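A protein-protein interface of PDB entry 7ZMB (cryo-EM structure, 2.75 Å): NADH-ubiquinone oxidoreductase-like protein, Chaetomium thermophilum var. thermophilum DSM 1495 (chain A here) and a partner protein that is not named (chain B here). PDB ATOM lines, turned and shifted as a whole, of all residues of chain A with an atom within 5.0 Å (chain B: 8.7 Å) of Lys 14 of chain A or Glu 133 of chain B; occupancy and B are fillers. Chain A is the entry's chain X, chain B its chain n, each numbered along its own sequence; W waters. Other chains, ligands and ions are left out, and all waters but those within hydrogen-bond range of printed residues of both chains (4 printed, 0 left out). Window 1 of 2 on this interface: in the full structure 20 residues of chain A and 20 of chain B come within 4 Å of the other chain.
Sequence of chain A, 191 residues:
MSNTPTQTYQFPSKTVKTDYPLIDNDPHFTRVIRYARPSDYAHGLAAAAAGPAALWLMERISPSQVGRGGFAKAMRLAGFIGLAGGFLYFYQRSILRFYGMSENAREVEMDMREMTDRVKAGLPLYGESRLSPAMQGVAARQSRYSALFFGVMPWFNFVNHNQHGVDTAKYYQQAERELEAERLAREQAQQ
The side-chain amino group (NZ) of Lys 14 of chain A is in hydrogen-bond range of the backbone carbonyl oxygen (O) of Leu 129 of chain B, at 3.1 Å. The backbone NH (N) of Lys 14 of chain A lies within hydrogen-bond range of the side-chain carboxylate (OE2) of Glu 133 of chain B (3.4 Å). The guanidinium group (NE) of Arg 141 of chain A is in hydrogen-bond range of the side-chain hydroxyl (OH) of Tyr 131 of chain B, at 3.2 Å. The guanidinium group (NH2) of Arg 141 of chain A sits at hydrogen-bond distance from the backbone carbonyl oxygen (O) of Ser 136 of chain B, 3.4 Å away. The guanidinium group (NH2) of Arg 144 of chain A is in salt-bridge range of the side-chain carboxylate (OE1) of Glu 133 of chain B (2.8 Å). O of Val 16 of chain A sits close to OE2 of Glu 165 of chain B (3.1 Å).
Water W4 lies within hydrogen-bond range of OG1 of Thr 15 of chain A (2.7 Å), O of Ser 13 of chain A (2.9 Å), O of Tyr 158 of chain B (2.9 Å) and NE2 of Gln 161 of chain B (3.3 Å). Water W1 lies within hydrogen-bond range of N of Thr 15 of chain A (2.8 Å), NE2 of Gln 161 of chain B (3.2 Å) and O of Ser 13 of chain A (3.2 Å). Water W3 lies within hydrogen-bond range of OG of Ser 136 of chain B (2.9 Å) and O of Pro 12 of chain A (3.0 Å). Water W2 lies within hydrogen-bond range of the backbone carbonyl oxygen (O) of Leu 129 of chain B (3.1 Å) and the side-chain amino group (NZ) of Lys 14 of chain A (3.4 Å).
Of the 10 printed residues of chain A, 7 touch a printed residue of chain B. Printed residues of chain B that touch a printed residue of chain A: Leu 129, Lys 130, Tyr 131, Pro 132, Glu 133, Phe 135, Ser 136, His 137, Ile 155, Tyr 158, Gln 161, His 162 and Glu 165. Among the printed residues, Asp or Glu carboxylates within 4 Å of a Lys or Arg side-chain nitrogen of the other chain: Arg 144 of chain A with Glu 133 of chain B (2.8 Å).
Among the printed residues, pairs that only touch across the chains: Ser 13 of chain A with Glu 133 of chain B, Pro 12 of chain A with Ser 136 of chain B, Arg 144 of chain A with Tyr 131 of chain B, Arg 141 of chain A with Glu 133 of chain B, Pro 12 of chain A with Glu 133 of chain B, Pro 12 of chain A with Pro 132 of chain B, Arg 141 of chain A with His 137 of chain B, Pro 12 of chain A with Ile 155 of chain B, Lys 14 of chain A with Lys 130 of chain B, Thr 15 of chain A with His 162 of chain B, Pro 12 of chain A with Tyr 158 of chain B, Thr 15 of chain A with Gln 161 of chain B, Arg 144 of chain A with Lys 130 of chain B, Pro 12 of chain A with Phe 135 of chain B, Thr 15 of chain A with Glu 165 of chain B and Lys 14 of chain A with Pro 132 of chain B.
Of chain B, only Leu 129 (3.1 Å), Lys 130 (3.5 Å), Pro 132 (3.8 Å) and Glu 133 (3.4 Å) come within 4 Å of Lys 14 of chain A. Of chain A, only Pro 12, Ser 13, Lys 14, Arg 141 and Arg 144 come within 4 Å of Glu 133 of chain B. Of the printed residues of chain A, Glu 165 of chain B touches Thr 15 and Val 16. Of the printed residues of chain A, Ser 136 of chain B touches Pro 12 (3.4 Å) and Arg 141 (3.4 Å). Printed residues of chain A within 4 Å of Tyr 131 of chain B: Arg 141 (3.2 Å) and Arg 144 (3.4 Å). Printed residues of chain A within 4 Å of Lys 130 of chain B: Lys 14 (3.5 Å) and Arg 144 (3.6 Å). Gln 163 of chain A touches none of the printed residues of chain B.
OE1 of Gln 161 of chain B lies close to OE2 of Glu 128 of chain B, at 3.1 Å. The side-chain hydroxyl of Tyr 131 of chain B sits at hydrogen-bond distance from a ring nitrogen (NE2) of His 137 of chain B (2.8 Å).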
ATOM      1  N   PRO A  12      -7.765  26.286  21.670  1.00  0.00           N
ATOM      2  CA  PRO A  12      -8.461  27.132  22.635  1.00  0.00           C
ATOM      3  C   PRO A  12      -9.973  27.051  22.402  1.00  0.00           C
ATOM      4  O   PRO A  12     -10.394  27.164  21.282  1.00  0.00           O
ATOM      5  CB  PRO A  12      -7.836  28.506  22.367  1.00  0.00           C
ATOM      6  CG  PRO A  12      -7.489  28.492  20.899  1.00  0.00           C
ATOM      7  CD  PRO A  12      -7.109  27.058  20.612  1.00  0.00           C
ATOM      8  N   SER A  13     -10.754  26.856  23.463  1.00  0.00           N
ATOM      9  CA  SER A  13     -12.190  26.681  23.320  1.00  0.00           C
ATOM     10  C   SER A  13     -12.920  27.632  24.250  1.00  0.00           C
ATOM     11  O   SER A  13     -12.393  28.052  25.280  1.00  0.00           O
ATOM     12  CB  SER A  13     -12.613  25.236  23.603  1.00  0.00           C
ATOM     13  OG  SER A  13     -12.731  25.004  24.993  1.00  0.00           O
ATOM     14  N   LYS A  14     -14.167  27.944  23.899  1.00  0.00           N
ATOM     15  CA  LYS A  14     -14.992  28.866  24.722  1.00  0.00           C
ATOM     16  C   LYS A  14     -15.533  28.123  25.939  1.00  0.00           C
ATOM     17  O   LYS A  14     -16.040  27.008  25.763  1.00  0.00           O
ATOM     18  CB  LYS A  14     -16.137  29.455  23.900  1.00  0.00           C
ATOM     19  CG  LYS A  14     -17.045  30.438  24.628  1.00  0.00           C
ATOM     20  CD  LYS A  14     -16.320  31.652  25.154  1.00  0.00           C
ATOM     21  CE  LYS A  14     -17.199  32.562  25.983  1.00  0.00           C
ATOM     22  NZ  LYS A  14     -16.442  33.735  26.480  1.00  0.00           N
ATOM     23  N   THR A  15     -15.383  28.722  27.124  1.00  0.00           N
ATOM     24  CA  THR A  15     -15.939  28.136  28.367  1.00  0.00           C
ATOM     25  C   THR A  15     -17.266  28.839  28.643  1.00  0.00           C
ATOM     26  O   THR A  15     -17.297  30.077  28.603  1.00  0.00           O
ATOM     27  CB  THR A  15     -14.931  28.224  29.518  1.00  0.00           C
ATOM     28  OG1 THR A  15     -14.002  27.156  29.337  1.00  0.00           O
ATOM     29  CG2 THR A  15     -15.568  28.112  30.885  1.00  0.00           C
ATOM     30  N   VAL A  16     -18.312  28.074  28.923  1.00  0.00           N
ATOM     31  CA  VAL A  16     -19.654  28.665  29.175  1.00  0.00           C
ATOM     32  C   VAL A  16     -20.069  28.277  30.593  1.00  0.00           C
ATOM     33  O   VAL A  16     -19.733  27.158  31.019  1.00  0.00           O
ATOM     34  CB  VAL A  16     -20.679  28.203  28.119  1.00  0.00           C
ATOM     35  CG1 VAL A  16     -21.982  28.976  28.220  1.00  0.00           C
ATOM     36  CG2 VAL A  16     -20.114  28.285  26.711  1.00  0.00           C
ATOM     37  N   ASN A  25     -18.876  19.996  22.858  1.00  0.00           N
ATOM     38  CA  ASN A  25     -19.473  21.240  22.305  1.00  0.00           C
ATOM     39  C   ASN A  25     -19.774  21.096  20.808  1.00  0.00           C
ATOM     40  O   ASN A  25     -20.511  21.938  20.288  1.00  0.00           O
ATOM     41  CB  ASN A  25     -18.653  22.479  22.676  1.00  0.00           C
ATOM     42  CG  ASN A  25     -17.285  22.597  22.040  1.00  0.00           C
ATOM     43  OD1 ASN A  25     -16.998  22.010  21.001  1.00  0.00           O
ATOM     44  ND2 ASN A  25     -16.433  23.398  22.652  1.00  0.00           N
ATOM     45  N   ARG A 141     -15.178  25.231  14.229  1.00  0.00           N
ATOM     46  CA  ARG A 141     -15.430  26.641  14.610  1.00  0.00           C
ATOM     47  C   ARG A 141     -16.704  27.155  13.947  1.00  0.00           C
ATOM     48  O   ARG A 141     -17.107  28.267  14.259  1.00  0.00           O
ATOM     49  CB  ARG A 141     -14.221  27.511  14.260  1.00  0.00           C
ATOM     50  CG  ARG A 141     -12.936  27.115  14.970  1.00  0.00           C
ATOM     51  CD  ARG A 141     -11.789  28.052  14.652  1.00  0.00           C
ATOM     52  NE  ARG A 141     -11.681  28.410  13.244  1.00  0.00           N
ATOM     53  CZ  ARG A 141     -10.768  27.935  12.405  1.00  0.00           C
ATOM     54  NH1 ARG A 141     -10.758  28.330  11.145  1.00  0.00           N
ATOM     55  NH2 ARG A 141      -9.862  27.076  12.829  1.00  0.00           N
ATOM     56  N   ARG A 144     -19.511  24.462  16.635  1.00  0.00           N
ATOM     57  CA  ARG A 144     -19.536  24.241  18.076  1.00  0.00           C
ATOM     58  C   ARG A 144     -20.559  25.174  18.721  1.00  0.00           C
ATOM     59  O   ARG A 144     -20.631  26.362  18.395  1.00  0.00           O
ATOM     60  CB  ARG A 144     -18.137  24.403  18.697  1.00  0.00           C
ATOM     61  CG  ARG A 144     -17.459  25.738  18.516  1.00  0.00           C
ATOM     62  CD  ARG A 144     -17.829  26.717  19.607  1.00  0.00           C
ATOM     63  NE  ARG A 144     -17.069  27.950  19.501  1.00  0.00           N
ATOM     64  CZ  ARG A 144     -17.294  29.020  20.241  1.00  0.00           C
ATOM     65  NH1 ARG A 144     -18.270  28.999  21.120  1.00  0.00           N
ATOM     66  NH2 ARG A 144     -16.578  30.117  20.077  1.00  0.00           N
ATOM     67  N   TYR A 145     -21.386  24.612  19.604  1.00  0.00           N
ATOM     68  CA  TYR A 145     -22.484  25.322  20.263  1.00  0.00           C
ATOM     69  C   TYR A 145     -23.503  25.867  19.269  1.00  0.00           C
ATOM     70  O   TYR A 145     -24.220  26.819  19.569  1.00  0.00           O
ATOM     71  CB  TYR A 145     -21.971  26.457  21.153  1.00  0.00           C
ATOM     72  CG  TYR A 145     -21.210  25.994  22.359  1.00  0.00           C
ATOM     73  CD1 TYR A 145     -21.758  25.081  23.240  1.00  0.00           C
ATOM     74  CD2 TYR A 145     -19.943  26.482  22.624  1.00  0.00           C
ATOM     75  CE1 TYR A 145     -21.066  24.660  24.341  1.00  0.00           C
ATOM     76  CE2 TYR A 145     -19.242  26.067  23.722  1.00  0.00           C
ATOM     77  CZ  TYR A 145     -19.805  25.154  24.576  1.00  0.00           C
ATOM     78  OH  TYR A 145     -19.099  24.745  25.676  1.00  0.00           O
ATOM     79  N   GLN A 163     -11.678  18.425  17.644  1.00  0.00           N
ATOM     80  CA  GLN A 163     -11.602  19.682  18.434  1.00  0.00           C
ATOM     81  C   GLN A 163     -12.974  19.834  19.090  1.00  0.00           C
ATOM     82  O   GLN A 163     -13.829  20.517  18.508  1.00  0.00           O
ATOM     83  CB  GLN A 163     -11.349  20.862  17.503  1.00  0.00           C
ATOM     84  CG  GLN A 163     -11.163  22.180  18.233  1.00  0.00           C
ATOM     85  CD  GLN A 163     -11.286  23.359  17.300  1.00  0.00           C
ATOM     86  OE1 GLN A 163     -10.525  23.502  16.350  1.00  0.00           O
ATOM     87  NE2 GLN A 163     -12.262  24.210  17.563  1.00  0.00           N
ATOM     88  N   ILE B 127     -12.298  42.599  28.674  1.00  0.00           N
ATOM     89  CA  ILE B 127     -13.080  41.941  27.593  1.00  0.00           C
ATOM     90  C   ILE B 127     -12.615  40.485  27.505  1.00  0.00           C
ATOM     91  O   ILE B 127     -11.416  40.259  27.355  1.00  0.00           O
ATOM     92  CB  ILE B 127     -12.858  42.698  26.268  1.00  0.00           C
ATOM     93  CG1 ILE B 127     -13.143  44.196  26.397  1.00  0.00           C
ATOM     94  CG2 ILE B 127     -13.653  42.065  25.136  1.00  0.00           C
ATOM     95  CD1 ILE B 127     -14.612  44.541  26.404  1.00  0.00           C
ATOM     96  N   GLU B 128     -13.552  39.538  27.563  1.00  0.00           N
ATOM     97  CA  GLU B 128     -13.234  38.094  27.416  1.00  0.00           C
ATOM     98  C   GLU B 128     -13.768  37.710  26.046  1.00  0.00           C
ATOM     99  O   GLU B 128     -14.933  38.019  25.793  1.00  0.00           O
ATOM    100  CB  GLU B 128     -13.941  37.272  28.495  1.00  0.00           C
ATOM    101  CG  GLU B 128     -13.140  36.087  28.988  1.00  0.00           C
ATOM    102  CD  GLU B 128     -13.409  35.690  30.427  1.00  0.00           C
ATOM    103  OE1 GLU B 128     -13.639  36.593  31.255  1.00  0.00           O
ATOM    104  OE2 GLU B 128     -13.391  34.478  30.719  1.00  0.00           O
ATOM    105  N   LEU B 129     -12.962  37.056  25.215  1.00  0.00           N
ATOM    106  CA  LEU B 129     -13.388  36.799  23.820  1.00  0.00           C
ATOM    107  C   LEU B 129     -14.605  35.880  23.722  1.00  0.00           C
ATOM    108  O   LEU B 129     -14.560  34.787  24.312  1.00  0.00           O
ATOM    109  CB  LEU B 129     -12.197  36.170  23.100  1.00  0.00           C
ATOM    110  CG  LEU B 129     -10.898  36.967  23.130  1.00  0.00           C
ATOM    111  CD1 LEU B 129      -9.841  36.287  22.277  1.00  0.00           C
ATOM    112  CD2 LEU B 129     -11.143  38.374  22.635  1.00  0.00           C
ATOM    113  N   LYS B 130     -15.663  36.325  23.044  1.00  0.00           N
ATOM    114  CA  LYS B 130     -16.822  35.454  22.729  1.00  0.00           C
ATOM    115  C   LYS B 130     -16.301  34.306  21.888  1.00  0.00           C
ATOM    116  O   LYS B 130     -16.810  33.191  22.020  1.00  0.00           O
ATOM    117  CB  LYS B 130     -17.859  36.239  21.929  1.00  0.00           C
ATOM    118  CG  LYS B 130     -18.635  37.302  22.687  1.00  0.00           C
ATOM    119  CD  LYS B 130     -19.421  38.200  21.765  1.00  0.00           C
ATOM    120  CE  LYS B 130     -20.480  39.006  22.481  1.00  0.00           C
ATOM    121  NZ  LYS B 130     -20.976  40.119  21.642  1.00  0.00           N
ATOM    122  N   TYR B 131     -15.340  34.612  21.025  1.00  0.00           N
ATOM    123  CA  TYR B 131     -14.764  33.605  20.111  1.00  0.00           C
ATOM    124  C   TYR B 131     -13.262  33.454  20.417  1.00  0.00           C
ATOM    125  O   TYR B 131     -12.465  34.051  19.690  1.00  0.00           O
ATOM    126  CB  TYR B 131     -15.188  33.994  18.702  1.00  0.00           C
ATOM    127  CG  TYR B 131     -14.752  33.102  17.575  1.00  0.00           C
ATOM    128  CD1 TYR B 131     -15.257  31.823  17.443  1.00  0.00           C
ATOM    129  CD2 TYR B 131     -13.887  33.572  16.605  1.00  0.00           C
ATOM    130  CE1 TYR B 131     -14.878  31.011  16.390  1.00  0.00           C
ATOM    131  CE2 TYR B 131     -13.505  32.778  15.544  1.00  0.00           C
ATOM    132  CZ  TYR B 131     -14.000  31.494  15.441  1.00  0.00           C
ATOM    133  OH  TYR B 131     -13.638  30.709  14.393  1.00  0.00           O
ATOM    134  N   PRO B 132     -12.818  32.706  21.461  1.00  0.00           N
ATOM    135  CA  PRO B 132     -11.391  32.457  21.704  1.00  0.00           C
ATOM    136  C   PRO B 132     -10.794  31.543  20.636  1.00  0.00           C
ATOM    137  O   PRO B 132      -9.653  31.229  20.761  1.00  0.00           O
ATOM    138  CB  PRO B 132     -11.371  31.614  22.988  1.00  0.00           C
ATOM    139  CG  PRO B 132     -12.650  31.944  23.676  1.00  0.00           C
ATOM    140  CD  PRO B 132     -13.612  32.035  22.518  1.00  0.00           C
ATOM    141  N   GLU B 133     -11.576  31.166  19.625  1.00  0.00           N
ATOM    142  CA  GLU B 133     -11.147  30.188  18.597  1.00  0.00           C
ATOM    143  C   GLU B 133     -10.501  30.970  17.459  1.00  0.00           C
ATOM    144  O   GLU B 133     -10.055  30.336  16.502  1.00  0.00           O
ATOM    145  CB  GLU B 133     -12.393  29.432  18.130  1.00  0.00           C
ATOM    146  CG  GLU B 133     -12.691  28.147  18.874  1.00  0.00           C
ATOM    147  CD  GLU B 133     -13.582  28.262  20.093  1.00  0.00           C
ATOM    148  OE1 GLU B 133     -13.872  29.395  20.501  1.00  0.00           O
ATOM    149  OE2 GLU B 133     -13.986  27.212  20.621  1.00  0.00           O
ATOM    150  N   VAL B 134     -10.486  32.298  17.560  1.00  0.00           N
ATOM    151  CA  VAL B 134      -9.791  33.168  16.570  1.00  0.00           C
ATOM    152  C   VAL B 134      -8.299  32.901  16.738  1.00  0.00           C
ATOM    153  O   VAL B 134      -7.528  33.301  15.855  1.00  0.00           O
ATOM    154  CB  VAL B 134     -10.119  34.651  16.830  1.00  0.00           C
ATOM    155  CG1 VAL B 134      -9.453  35.183  18.091  1.00  0.00           C
ATOM    156  CG2 VAL B 134      -9.832  35.544  15.638  1.00  0.00           C
ATOM    157  N   PHE B 135      -7.898  32.179  17.785  1.00  0.00           N
ATOM    158  CA  PHE B 135      -6.460  31.926  18.051  1.00  0.00           C
ATOM    159  C   PHE B 135      -6.027  30.753  17.184  1.00  0.00           C
ATOM    160  O   PHE B 135      -4.837  30.418  17.185  1.00  0.00           O
ATOM    161  CB  PHE B 135      -6.205  31.643  19.531  1.00  0.00           C
ATOM    162  CG  PHE B 135      -6.030  32.835  20.433  1.00  0.00           C
ATOM    163  CD1 PHE B 135      -4.909  33.640  20.335  1.00  0.00           C
ATOM    164  CD2 PHE B 135      -6.961  33.117  21.419  1.00  0.00           C
ATOM    165  CE1 PHE B 135      -4.736  34.718  21.186  1.00  0.00           C
ATOM    166  CE2 PHE B 135      -6.791  34.202  22.265  1.00  0.00           C
ATOM    167  CZ  PHE B 135      -5.674  34.995  22.150  1.00  0.00           C
ATOM    168  N   SER B 136      -6.976  30.164  16.461  1.00  0.00           N
ATOM    169  CA  SER B 136      -6.699  28.978  15.613  1.00  0.00           C
ATOM    170  C   SER B 136      -6.858  29.366  14.144  1.00  0.00           C
ATOM    171  O   SER B 136      -6.763  28.474  13.284  1.00  0.00           O
ATOM    172  CB  SER B 136      -7.612  27.879  15.992  1.00  0.00           C
ATOM    173  OG  SER B 136      -7.264  27.334  17.253  1.00  0.00           O
ATOM    174  N   HIS B 137      -7.064  30.659  13.884  1.00  0.00           N
ATOM    175  CA  HIS B 137      -7.214  31.189  12.505  1.00  0.00           C
ATOM    176  C   HIS B 137      -5.861  31.310  11.803  1.00  0.00           C
ATOM    177  O   HIS B 137      -4.822  31.145  12.468  1.00  0.00           O
ATOM    178  CB  HIS B 137      -7.904  32.559  12.536  1.00  0.00           C
ATOM    179  CG  HIS B 137      -9.379  32.500  12.723  1.00  0.00           C
ATOM    180  ND1 HIS B 137     -10.214  33.507  12.287  1.00  0.00           N
ATOM    181  CD2 HIS B 137     -10.172  31.565  13.285  1.00  0.00           C
ATOM    182  CE1 HIS B 137     -11.458  33.199  12.579  1.00  0.00           C
ATOM    183  NE2 HIS B 137     -11.456  32.014  13.188  1.00  0.00           N
ATOM    184  N   GLY B 138      -5.884  31.594  10.504  1.00  0.00           N
ATOM    185  CA  GLY B 138      -4.649  31.728   9.708  1.00  0.00           C
ATOM    186  C   GLY B 138      -4.585  30.713   8.594  1.00  0.00           C
ATOM    187  O   GLY B 138      -4.979  29.570   8.833  1.00  0.00           O
ATOM    188  N   VAL B 154      -1.445  30.744  25.796  1.00  0.00           N
ATOM    189  CA  VAL B 154      -2.901  31.010  25.607  1.00  0.00           C
ATOM    190  C   VAL B 154      -3.662  29.688  25.765  1.00  0.00           C
ATOM    191  O   VAL B 154      -4.706  29.686  26.424  1.00  0.00           O
ATOM    192  CB  VAL B 154      -3.185  31.661  24.238  1.00  0.00           C
ATOM    193  CG1 VAL B 154      -4.571  32.262  24.189  1.00  0.00           C
ATOM    194  CG2 VAL B 154      -2.138  32.702  23.890  1.00  0.00           C
ATOM    195  N   ILE B 155      -3.136  28.611  25.185  1.00  0.00           N
ATOM    196  CA  ILE B 155      -3.814  27.289  25.258  1.00  0.00           C
ATOM    197  C   ILE B 155      -3.830  26.845  26.721  1.00  0.00           C
ATOM    198  O   ILE B 155      -4.846  26.287  27.150  1.00  0.00           O
ATOM    199  CB  ILE B 155      -3.179  26.258  24.297  1.00  0.00           C
ATOM    200  CG1 ILE B 155      -2.799  26.873  22.949  1.00  0.00           C
ATOM    201  CG2 ILE B 155      -4.094  25.061  24.114  1.00  0.00           C
ATOM    202  CD1 ILE B 155      -3.968  27.389  22.155  1.00  0.00           C
ATOM    203  N   TYR B 158      -6.614  28.759  28.496  1.00  0.00           N
ATOM    204  CA  TYR B 158      -7.955  28.250  28.115  1.00  0.00           C
ATOM    205  C   TYR B 158      -8.192  26.871  28.729  1.00  0.00           C
ATOM    206  O   TYR B 158      -9.325  26.592  29.142  1.00  0.00           O
ATOM    207  CB  TYR B 158      -8.218  28.422  26.619  1.00  0.00           C
ATOM    208  CG  TYR B 158      -8.509  29.843  26.215  1.00  0.00           C
ATOM    209  CD1 TYR B 158      -9.588  30.525  26.748  1.00  0.00           C
ATOM    210  CD2 TYR B 158      -7.707  30.507  25.305  1.00  0.00           C
ATOM    211  CE1 TYR B 158      -9.860  31.835  26.390  1.00  0.00           C
ATOM    212  CE2 TYR B 158      -7.969  31.812  24.929  1.00  0.00           C
ATOM    213  CZ  TYR B 158      -9.049  32.479  25.475  1.00  0.00           C
ATOM    214  OH  TYR B 158      -9.318  33.761  25.102  1.00  0.00           O
ATOM    215  N   GLN B 161      -9.209  27.439  32.337  1.00  0.00           N
ATOM    216  CA  GLN B 161     -10.613  27.902  32.446  1.00  0.00           C
ATOM    217  C   GLN B 161     -11.546  26.695  32.301  1.00  0.00           C
ATOM    218  O   GLN B 161     -12.456  26.574  33.138  1.00  0.00           O
ATOM    219  CB  GLN B 161     -10.881  29.035  31.455  1.00  0.00           C
ATOM    220  CG  GLN B 161     -12.206  29.749  31.658  1.00  0.00           C
ATOM    221  CD  GLN B 161     -12.462  30.759  30.566  1.00  0.00           C
ATOM    222  OE1 GLN B 161     -13.520  31.379  30.501  1.00  0.00           O
ATOM    223  NE2 GLN B 161     -11.486  30.929  29.690  1.00  0.00           N
ATOM    224  N   HIS B 162     -11.340  25.845  31.290  1.00  0.00           N
ATOM    225  CA  HIS B 162     -12.176  24.624  31.148  1.00  0.00           C
ATOM    226  C   HIS B 162     -12.066  23.722  32.383  1.00  0.00           C
ATOM    227  O   HIS B 162     -13.117  23.399  32.942  1.00  0.00           O
ATOM    228  CB  HIS B 162     -11.817  23.854  29.866  1.00  0.00           C
ATOM    229  CG  HIS B 162     -12.477  22.524  29.737  1.00  0.00           C
ATOM    230  ND1 HIS B 162     -13.827  22.387  29.507  1.00  0.00           N
ATOM    231  CD2 HIS B 162     -11.972  21.276  29.780  1.00  0.00           C
ATOM    232  CE1 HIS B 162     -14.130  21.108  29.430  1.00  0.00           C
ATOM    233  NE2 HIS B 162     -13.011  20.406  29.599  1.00  0.00           N
ATOM    234  N   GLU B 165     -13.933  25.439  35.516  1.00  0.00           N
ATOM    235  CA  GLU B 165     -15.410  25.490  35.359  1.00  0.00           C
ATOM    236  C   GLU B 165     -15.963  24.086  35.591  1.00  0.00           C
ATOM    237  O   GLU B 165     -16.984  23.968  36.277  1.00  0.00           O
ATOM    238  CB  GLU B 165     -15.754  26.003  33.955  1.00  0.00           C
ATOM    239  CG  GLU B 165     -17.181  25.738  33.520  1.00  0.00           C
ATOM    240  CD  GLU B 165     -18.212  26.747  33.988  1.00  0.00           C
ATOM    241  OE1 GLU B 165     -17.818  27.874  34.347  1.00  0.00           O
ATOM    242  OE2 GLU B 165     -19.410  26.405  33.985  1.00  0.00           O
ATOM    243  N   GLU B 166     -15.284  23.067  35.060  1.00  0.00           N
ATOM    244  CA  GLU B 166     -15.738  21.656  35.169  1.00  0.00           C
ATOM    245  C   GLU B 166     -15.526  21.205  36.609  1.00  0.00           C
ATOM    246  O   GLU B 166     -16.375  20.483  37.131  1.00  0.00           O
ATOM    247  CB  GLU B 166     -14.960  20.767  34.196  1.00  0.00           C
ATOM    248  CG  GLU B 166     -15.174  21.106  32.734  1.00  0.00           C
ATOM    249  CD  GLU B 166     -16.608  21.179  32.241  1.00  0.00           C
ATOM    250  OE1 GLU B 166     -17.447  20.393  32.719  1.00  0.00           O
ATOM    251  OE2 GLU B 166     -16.881  22.030  31.373  1.00  0.00           O
HETATM  252  O   HOH W   1     -13.308  30.600  27.052  1.00  0.00           O
HETATM  253  O   HOH W   2     -13.051  33.718  26.769  1.00  0.00           O
HETATM  254  O   HOH W   3      -9.969  26.846  18.286  1.00  0.00           O
HETATM  255  O   HOH W   4     -11.697  28.028  28.138  1.00  0.00           O
